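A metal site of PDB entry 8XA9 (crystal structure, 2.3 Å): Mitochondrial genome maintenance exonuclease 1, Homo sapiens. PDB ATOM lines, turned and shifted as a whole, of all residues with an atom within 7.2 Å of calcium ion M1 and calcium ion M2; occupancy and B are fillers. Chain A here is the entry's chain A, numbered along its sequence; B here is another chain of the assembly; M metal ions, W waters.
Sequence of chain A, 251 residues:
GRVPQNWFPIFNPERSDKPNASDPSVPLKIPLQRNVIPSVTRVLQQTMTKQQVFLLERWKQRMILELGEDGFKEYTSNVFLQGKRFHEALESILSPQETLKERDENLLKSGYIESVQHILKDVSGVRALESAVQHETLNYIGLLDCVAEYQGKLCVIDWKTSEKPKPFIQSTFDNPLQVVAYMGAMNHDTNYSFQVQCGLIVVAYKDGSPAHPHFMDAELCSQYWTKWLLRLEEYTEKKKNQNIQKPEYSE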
ATOM      1  N   HIS A  87     -34.657 -11.696   0.538  1.00  0.00           N
ATOM      2  CA  HIS A  87     -34.253 -11.146  -0.750  1.00  0.00           C
ATOM      3  C   HIS A  87     -35.387 -11.242  -1.764  1.00  0.00           C
ATOM      4  O   HIS A  87     -35.634 -10.296  -2.525  1.00  0.00           O
ATOM      5  CB  HIS A  87     -33.013 -11.871  -1.271  1.00  0.00           C
ATOM      6  CG  HIS A  87     -31.720 -11.335  -0.712  1.00  0.00           C
ATOM      7  ND1 HIS A  87     -31.301 -11.585   0.568  1.00  0.00           N
ATOM      8  CD2 HIS A  87     -30.756 -10.572  -1.283  1.00  0.00           C
ATOM      9  CE1 HIS A  87     -30.135 -10.992   0.770  1.00  0.00           C
ATOM     10  NE2 HIS A  87     -29.785 -10.370  -0.341  1.00  0.00           N
ATOM     11  N   GLU A 130     -32.089  -8.393  -8.893  1.00  0.00           N
ATOM     12  CA  GLU A 130     -31.564  -9.745  -9.061  1.00  0.00           C
ATOM     13  C   GLU A 130     -31.065  -9.971 -10.493  1.00  0.00           C
ATOM     14  O   GLU A 130     -31.368 -10.958 -11.148  1.00  0.00           O
ATOM     15  CB  GLU A 130     -32.619 -10.789  -8.696  1.00  0.00           C
ATOM     16  CG  GLU A 130     -33.004 -10.793  -7.225  1.00  0.00           C
ATOM     17  CD  GLU A 130     -31.919 -11.394  -6.341  1.00  0.00           C
ATOM     18  OE1 GLU A 130     -30.927 -11.925  -6.879  1.00  0.00           O
ATOM     19  OE2 GLU A 130     -32.060 -11.332  -5.099  1.00  0.00           O
ATOM     20  N   LEU A 143     -24.533 -11.656  -9.489  1.00  0.00           N
ATOM     21  CA  LEU A 143     -25.951 -11.296  -9.455  1.00  0.00           C
ATOM     22  C   LEU A 143     -26.154 -10.262  -8.367  1.00  0.00           C
ATOM     23  O   LEU A 143     -26.112 -10.591  -7.177  1.00  0.00           O
ATOM     24  CB  LEU A 143     -26.828 -12.517  -9.193  1.00  0.00           C
ATOM     25  CG  LEU A 143     -27.169 -13.433 -10.375  1.00  0.00           C
ATOM     26  CD1 LEU A 143     -27.760 -14.742  -9.862  1.00  0.00           C
ATOM     27  CD2 LEU A 143     -28.118 -12.755 -11.344  1.00  0.00           C
ATOM     28  N   LEU A 144     -26.368  -9.009  -8.765  1.00  0.00           N
ATOM     29  CA  LEU A 144     -26.600  -7.953  -7.786  1.00  0.00           C
ATOM     30  C   LEU A 144     -28.052  -7.957  -7.321  1.00  0.00           C
ATOM     31  O   LEU A 144     -28.960  -8.279  -8.081  1.00  0.00           O
ATOM     32  CB  LEU A 144     -26.235  -6.586  -8.361  1.00  0.00           C
ATOM     33  CG  LEU A 144     -26.824  -6.175  -9.723  1.00  0.00           C
ATOM     34  CD1 LEU A 144     -28.239  -5.643  -9.575  1.00  0.00           C
ATOM     35  CD2 LEU A 144     -25.931  -5.135 -10.385  1.00  0.00           C
ATOM     36  N   ASP A 145     -28.252  -7.609  -6.057  1.00  0.00           N
ATOM     37  CA  ASP A 145     -29.602  -7.588  -5.495  1.00  0.00           C
ATOM     38  C   ASP A 145     -30.452  -6.523  -6.168  1.00  0.00           C
ATOM     39  O   ASP A 145     -31.508  -6.817  -6.751  1.00  0.00           O
ATOM     40  CB  ASP A 145     -29.538  -7.344  -3.994  1.00  0.00           C
ATOM     41  CG  ASP A 145     -28.934  -8.500  -3.229  1.00  0.00           C
ATOM     42  OD1 ASP A 145     -28.855  -9.612  -3.803  1.00  0.00           O
ATOM     43  OD2 ASP A 145     -28.554  -8.299  -2.058  1.00  0.00           O
ATOM     44  N   ILE A 157     -27.568  -1.855  -4.423  1.00  0.00           N
ATOM     45  CA  ILE A 157     -27.919  -2.091  -3.036  1.00  0.00           C
ATOM     46  C   ILE A 157     -27.741  -3.561  -2.720  1.00  0.00           C
ATOM     47  O   ILE A 157     -28.026  -4.424  -3.555  1.00  0.00           O
ATOM     48  CB  ILE A 157     -29.369  -1.635  -2.739  1.00  0.00           C
ATOM     49  CG1 ILE A 157     -29.547  -0.160  -3.136  1.00  0.00           C
ATOM     50  CG2 ILE A 157     -29.707  -1.826  -1.272  1.00  0.00           C
ATOM     51  CD1 ILE A 157     -30.965   0.352  -3.042  1.00  0.00           C
ATOM     52  N   ASP A 158     -27.255  -3.852  -1.518  1.00  0.00           N
ATOM     53  CA  ASP A 158     -27.028  -5.213  -1.039  1.00  0.00           C
ATOM     54  C   ASP A 158     -27.849  -5.413   0.229  1.00  0.00           C
ATOM     55  O   ASP A 158     -27.406  -5.038   1.320  1.00  0.00           O
ATOM     56  CB  ASP A 158     -25.552  -5.477  -0.791  1.00  0.00           C
ATOM     57  CG  ASP A 158     -25.301  -6.800  -0.090  1.00  0.00           C
ATOM     58  OD1 ASP A 158     -26.177  -7.693  -0.163  1.00  0.00           O
ATOM     59  OD2 ASP A 158     -24.228  -6.971   0.518  1.00  0.00           O
ATOM     60  N   TRP A 159     -29.034  -6.007   0.097  1.00  0.00           N
ATOM     61  CA  TRP A 159     -29.815  -6.355   1.266  1.00  0.00           C
ATOM     62  C   TRP A 159     -29.196  -7.562   1.971  1.00  0.00           C
ATOM     63  O   TRP A 159     -28.431  -8.331   1.376  1.00  0.00           O
ATOM     64  CB  TRP A 159     -31.264  -6.693   0.905  1.00  0.00           C
ATOM     65  CG  TRP A 159     -31.818  -5.943  -0.272  1.00  0.00           C
ATOM     66  CD1 TRP A 159     -31.958  -6.418  -1.542  1.00  0.00           C
ATOM     67  CD2 TRP A 159     -32.325  -4.610  -0.281  1.00  0.00           C
ATOM     68  NE1 TRP A 159     -32.514  -5.453  -2.343  1.00  0.00           N
ATOM     69  CE2 TRP A 159     -32.753  -4.334  -1.586  1.00  0.00           C
ATOM     70  CE3 TRP A 159     -32.461  -3.611   0.699  1.00  0.00           C
ATOM     71  CZ2 TRP A 159     -33.299  -3.104  -1.950  1.00  0.00           C
ATOM     72  CZ3 TRP A 159     -32.999  -2.404   0.340  1.00  0.00           C
ATOM     73  CH2 TRP A 159     -33.418  -2.156  -0.980  1.00  0.00           C
ATOM     74  N   LYS A 160     -29.543  -7.727   3.250  1.00  0.00           N
ATOM     75  CA  LYS A 160     -29.163  -8.930   3.974  1.00  0.00           C
ATOM     76  C   LYS A 160     -29.770  -8.947   5.379  1.00  0.00           C
ATOM     77  O   LYS A 160     -29.963  -7.896   5.992  1.00  0.00           O
ATOM     78  CB  LYS A 160     -27.638  -9.060   4.085  1.00  0.00           C
ATOM     79  CG  LYS A 160     -26.953  -7.924   4.833  1.00  0.00           C
ATOM     80  CD  LYS A 160     -25.457  -8.186   5.062  1.00  0.00           C
ATOM     81  CE  LYS A 160     -24.798  -9.015   3.956  1.00  0.00           C
ATOM     82  NZ  LYS A 160     -24.753  -8.294   2.657  1.00  0.00           N
ATOM     83  N   THR A 161     -30.063 -10.150   5.864  1.00  0.00           N
ATOM     84  CA  THR A 161     -30.462 -10.351   7.247  1.00  0.00           C
ATOM     85  C   THR A 161     -29.224 -10.619   8.093  1.00  0.00           C
ATOM     86  O   THR A 161     -28.146 -10.927   7.587  1.00  0.00           O
ATOM     87  CB  THR A 161     -31.436 -11.517   7.366  1.00  0.00           C
ATOM     88  OG1 THR A 161     -30.811 -12.714   6.872  1.00  0.00           O
ATOM     89  CG2 THR A 161     -32.694 -11.245   6.561  1.00  0.00           C
ATOM     90  N   ASN A 175     -18.774  -7.654   2.565  1.00  0.00           N
ATOM     91  CA  ASN A 175     -19.893  -7.132   1.788  1.00  0.00           C
ATOM     92  C   ASN A 175     -19.548  -5.892   0.975  1.00  0.00           C
ATOM     93  O   ASN A 175     -20.008  -5.804  -0.182  1.00  0.00           O
ATOM     94  CB  ASN A 175     -21.070  -6.827   2.730  1.00  0.00           C
ATOM     95  CG  ASN A 175     -21.596  -8.073   3.428  1.00  0.00           C
ATOM     96  OD1 ASN A 175     -21.998  -8.017   4.584  1.00  0.00           O
ATOM     97  ND2 ASN A 175     -21.618  -9.191   2.709  1.00  0.00           N
ATOM     98  N   GLN A 178     -18.025  -7.124  -2.162  1.00  0.00           N
ATOM     99  CA  GLN A 178     -19.042  -7.694  -3.031  1.00  0.00           C
ATOM    100  C   GLN A 178     -19.810  -6.603  -3.769  1.00  0.00           C
ATOM    101  O   GLN A 178     -20.178  -6.776  -4.934  1.00  0.00           O
ATOM    102  CB  GLN A 178     -20.002  -8.564  -2.216  1.00  0.00           C
ATOM    103  CG  GLN A 178     -20.927  -9.406  -3.084  1.00  0.00           C
ATOM    104  CD  GLN A 178     -21.802 -10.343  -2.270  1.00  0.00           C
ATOM    105  OE1 GLN A 178     -21.480 -10.682  -1.130  1.00  0.00           O
ATOM    106  NE2 GLN A 178     -22.909 -10.787  -2.851  1.00  0.00           N
ATOM    107  N   TYR A 182     -19.822  -5.667  -7.928  1.00  0.00           N
ATOM    108  CA  TYR A 182     -21.031  -5.550  -8.741  1.00  0.00           C
ATOM    109  C   TYR A 182     -21.051  -4.232  -9.502  1.00  0.00           C
ATOM    110  O   TYR A 182     -21.386  -4.207 -10.701  1.00  0.00           O
ATOM    111  CB  TYR A 182     -22.279  -5.675  -7.870  1.00  0.00           C
ATOM    112  CG  TYR A 182     -22.513  -7.046  -7.274  1.00  0.00           C
ATOM    113  CD1 TYR A 182     -22.167  -8.207  -7.957  1.00  0.00           C
ATOM    114  CD2 TYR A 182     -23.109  -7.187  -6.024  1.00  0.00           C
ATOM    115  CE1 TYR A 182     -22.394  -9.457  -7.410  1.00  0.00           C
ATOM    116  CE2 TYR A 182     -23.335  -8.429  -5.465  1.00  0.00           C
ATOM    117  CZ  TYR A 182     -22.977  -9.568  -6.164  1.00  0.00           C
ATOM    118  OH  TYR A 182     -23.193 -10.808  -5.615  1.00  0.00           O
ATOM    119  N   VAL A 202     -27.694  -2.714   3.392  1.00  0.00           N
ATOM    120  CA  VAL A 202     -28.816  -2.626   4.324  1.00  0.00           C
ATOM    121  C   VAL A 202     -28.853  -3.907   5.132  1.00  0.00           C
ATOM    122  O   VAL A 202     -28.994  -5.005   4.568  1.00  0.00           O
ATOM    123  CB  VAL A 202     -30.147  -2.403   3.591  1.00  0.00           C
ATOM    124  CG1 VAL A 202     -31.297  -2.424   4.574  1.00  0.00           C
ATOM    125  CG2 VAL A 202     -30.119  -1.095   2.809  1.00  0.00           C
ATOM    126  P    DT B   2     -21.644 -20.095 -10.303  1.00  0.00           P
ATOM    127  OP1  DT B   2     -20.599 -19.433 -11.126  1.00  0.00           O
ATOM    128  OP2  DT B   2     -21.254 -21.020  -9.221  1.00  0.00           O
ATOM    129  O5'  DT B   2     -22.585 -18.980  -9.634  1.00  0.00           O
ATOM    130  C5'  DT B   2     -23.022 -17.875 -10.407  1.00  0.00           C
ATOM    131  C4'  DT B   2     -23.937 -16.971  -9.605  1.00  0.00           C
ATOM    132  O4'  DT B   2     -25.159 -17.683  -9.261  1.00  0.00           O
ATOM    133  C3'  DT B   2     -23.345 -16.478  -8.276  1.00  0.00           C
ATOM    134  O3'  DT B   2     -23.525 -15.070  -8.156  1.00  0.00           O
ATOM    135  C2'  DT B   2     -24.137 -17.255  -7.208  1.00  0.00           C
ATOM    136  C1'  DT B   2     -25.477 -17.456  -7.909  1.00  0.00           C
ATOM    137  N1   DT B   2     -26.278 -18.606  -7.399  1.00  0.00           N
ATOM    138  C2   DT B   2     -27.596 -18.401  -7.067  1.00  0.00           C
ATOM    139  O2   DT B   2     -28.151 -17.315  -7.153  1.00  0.00           O
ATOM    140  N3   DT B   2     -28.253 -19.511  -6.609  1.00  0.00           N
ATOM    141  C4   DT B   2     -27.741 -20.778  -6.466  1.00  0.00           C
ATOM    142  O4   DT B   2     -28.417 -21.716  -6.047  1.00  0.00           O
ATOM    143  C5   DT B   2     -26.350 -20.930  -6.838  1.00  0.00           C
ATOM    144  C7   DT B   2     -25.692 -22.265  -6.716  1.00  0.00           C
ATOM    145  C6   DT B   2     -25.694 -19.853  -7.281  1.00  0.00           C
ATOM    146  P    DT B   3     -22.890 -14.243  -6.938  1.00  0.00           P
ATOM    147  OP1  DT B   3     -22.902 -12.823  -7.323  1.00  0.00           O
ATOM    148  OP2  DT B   3     -21.601 -14.894  -6.570  1.00  0.00           O
ATOM    149  O5'  DT B   3     -23.934 -14.473  -5.749  1.00  0.00           O
ATOM    150  C5'  DT B   3     -25.308 -14.180  -5.971  1.00  0.00           C
ATOM    151  C4'  DT B   3     -26.183 -14.717  -4.848  1.00  0.00           C
ATOM    152  O4'  DT B   3     -26.254 -16.154  -4.935  1.00  0.00           O
ATOM    153  C3'  DT B   3     -25.694 -14.418  -3.424  1.00  0.00           C
ATOM    154  O3'  DT B   3     -26.544 -13.428  -2.829  1.00  0.00           O
ATOM    155  C2'  DT B   3     -25.757 -15.775  -2.692  1.00  0.00           C
ATOM    156  C1'  DT B   3     -26.584 -16.638  -3.644  1.00  0.00           C
ATOM    157  N1   DT B   3     -26.296 -18.099  -3.580  1.00  0.00           N
ATOM    158  C2   DT B   3     -27.348 -18.966  -3.345  1.00  0.00           C
ATOM    159  O2   DT B   3     -28.505 -18.603  -3.206  1.00  0.00           O
ATOM    160  N3   DT B   3     -27.000 -20.285  -3.294  1.00  0.00           N
ATOM    161  C4   DT B   3     -25.735 -20.817  -3.443  1.00  0.00           C
ATOM    162  O4   DT B   3     -25.520 -22.027  -3.383  1.00  0.00           O
ATOM    163  C5   DT B   3     -24.676 -19.858  -3.682  1.00  0.00           C
ATOM    164  C7   DT B   3     -23.266 -20.324  -3.858  1.00  0.00           C
ATOM    165  C6   DT B   3     -25.006 -18.560  -3.736  1.00  0.00           C
ATOM    166  P    DT B   4     -26.193 -12.816  -1.388  1.00  0.00           P
ATOM    167  OP1  DT B   4     -26.810 -11.478  -1.326  1.00  0.00           O
ATOM    168  OP2  DT B   4     -24.740 -12.973  -1.161  1.00  0.00           O
ATOM    169  O5'  DT B   4     -26.978 -13.769  -0.363  1.00  0.00           O
ATOM    170  C5'  DT B   4     -28.387 -13.974  -0.526  1.00  0.00           C
ATOM    171  C4'  DT B   4     -28.898 -15.028   0.442  1.00  0.00           C
ATOM    172  O4'  DT B   4     -28.611 -16.326  -0.084  1.00  0.00           O
ATOM    173  C3'  DT B   4     -28.248 -14.998   1.827  1.00  0.00           C
ATOM    174  O3'  DT B   4     -29.052 -14.232   2.727  1.00  0.00           O
ATOM    175  C2'  DT B   4     -28.161 -16.480   2.242  1.00  0.00           C
ATOM    176  C1'  DT B   4     -28.532 -17.255   0.974  1.00  0.00           C
ATOM    177  N1   DT B   4     -27.546 -18.323   0.579  1.00  0.00           N
ATOM    178  C2   DT B   4     -28.017 -19.571   0.239  1.00  0.00           C
ATOM    179  O2   DT B   4     -29.201 -19.877   0.253  1.00  0.00           O
ATOM    180  N3   DT B   4     -27.040 -20.474  -0.104  1.00  0.00           N
ATOM    181  C4   DT B   4     -25.680 -20.246  -0.151  1.00  0.00           C
ATOM    182  O4   DT B   4     -24.882 -21.129  -0.483  1.00  0.00           O
ATOM    183  C5   DT B   4     -25.264 -18.917   0.213  1.00  0.00           C
ATOM    184  C7   DT B   4     -23.805 -18.558   0.192  1.00  0.00           C
ATOM    185  C6   DT B   4     -26.202 -18.025   0.545  1.00  0.00           C
ATOM    186  P    DT B   5     -28.378 -13.122   3.673  1.00  0.00           P
ATOM    187  OP1  DT B   5     -29.478 -12.409   4.367  1.00  0.00           O
ATOM    188  OP2  DT B   5     -27.396 -12.368   2.867  1.00  0.00           O
ATOM    189  O5'  DT B   5     -27.571 -13.976   4.761  1.00  0.00           O
ATOM    190  C5'  DT B   5     -28.262 -14.589   5.841  1.00  0.00           C
ATOM    191  C4'  DT B   5     -27.411 -15.650   6.494  1.00  0.00           C
ATOM    192  O4'  DT B   5     -26.899 -16.559   5.494  1.00  0.00           O
ATOM    193  C3'  DT B   5     -26.179 -15.140   7.221  1.00  0.00           C
ATOM    194  O3'  DT B   5     -26.505 -14.724   8.548  1.00  0.00           O
ATOM    195  C2'  DT B   5     -25.253 -16.356   7.205  1.00  0.00           C
ATOM    196  C1'  DT B   5     -25.639 -17.062   5.899  1.00  0.00           C
ATOM    197  N1   DT B   5     -24.647 -16.856   4.807  1.00  0.00           N
ATOM    198  C2   DT B   5     -23.541 -17.657   4.738  1.00  0.00           C
ATOM    199  O2   DT B   5     -23.309 -18.540   5.551  1.00  0.00           O
ATOM    200  N3   DT B   5     -22.695 -17.389   3.697  1.00  0.00           N
ATOM    201  C4   DT B   5     -22.851 -16.420   2.727  1.00  0.00           C
ATOM    202  O4   DT B   5     -22.041 -16.256   1.819  1.00  0.00           O
ATOM    203  C5   DT B   5     -24.046 -15.613   2.848  1.00  0.00           C
ATOM    204  C7   DT B   5     -24.325 -14.528   1.848  1.00  0.00           C
ATOM    205  C6   DT B   5     -24.882 -15.866   3.861  1.00  0.00           C
HETATM  206 CA    CA M   1     -27.653  -9.563  -0.395  1.00  0.00          CA
HETATM  207 CA    CA M   2     -27.933 -11.768  -3.537  1.00  0.00          CA
HETATM  208  O   HOH W   1     -30.086 -12.990  -3.704  1.00  0.00           O
HETATM  209  O   HOH W   2     -25.709 -10.905  -3.926  1.00  0.00           O
HETATM  210  O   HOH W   3     -28.301 -11.997  -5.974  1.00  0.00           O
HETATM  211  O   HOH W   4     -26.560 -10.659   1.383  1.00  0.00           O
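The backbone NH of Val 202 lies within hydrogen-bond range of the backbone carbonyl oxygen of Asp 158.
The backbone NH (N) of Leu 143 sits at hydrogen-bond distance from OP1 of DT 3 of chain B (3.0 Å).
OP1 of DT 3 of chain B lies within hydrogen-bond range of the side-chain hydroxyl (OH) of Tyr 182 (2.7 Å).
The side-chain carboxylate (OD2) of Asp 158 lies within salt-bridge range of the side-chain amino group (NZ) of Lys 160, 2.6 Å away.
OP2 of DT 4 of chain B sits at hydrogen-bond distance from NE2 of Gln 178 (3.3 Å).
O of Asp 145 lies within hydrogen-bond range of N of Glu 130 (2.7 Å).
Of the 18 residues printed, 5 come within 4 Å of calcium ion M1.
The nearest printed residue that does not touch calcium ion M1 is DT 5 of chain B (4.3 Å).
Of the 18 residues printed, 4 come within 4 Å of calcium ion M2.
The nearest printed residue that does not touch calcium ion M2 is Leu 143 (4.2 Å).
Calcium ion M1 is bound by OD2 of Asp 145 (2.3 Å), NE2 of His 87 (2.3 Å), OP1 of DT 4 of chain B (2.3 Å), O of Trp 159 (2.3 Å), water W4 (2.4 Å) and OD1 of Asp 158 (2.4 Å).
Calcium ion M2 is bound by O3' of DT 3 of chain B (2.3 Å), OD1 of Asp 145 (2.4 Å), water W2 (2.4 Å), water W3 (2.5 Å), water W1 (2.5 Å) and OP1 of DT 4 of chain B (2.5 Å).
Water W4 bridges OP2 of DT 5 of chain B and the side-chain amino group (NZ) of Lys 160.
Water W2 lies within hydrogen-bond range of the side-chain amide nitrogen (NE2) of Gln 178, the side-chain hydroxyl (OH) of Tyr 182 and the backbone carbonyl oxygen (O) of Leu 143.
Water W3 bridges the side-chain carboxylate of Glu 130 and the backbone carbonyl oxygen of Leu 143.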
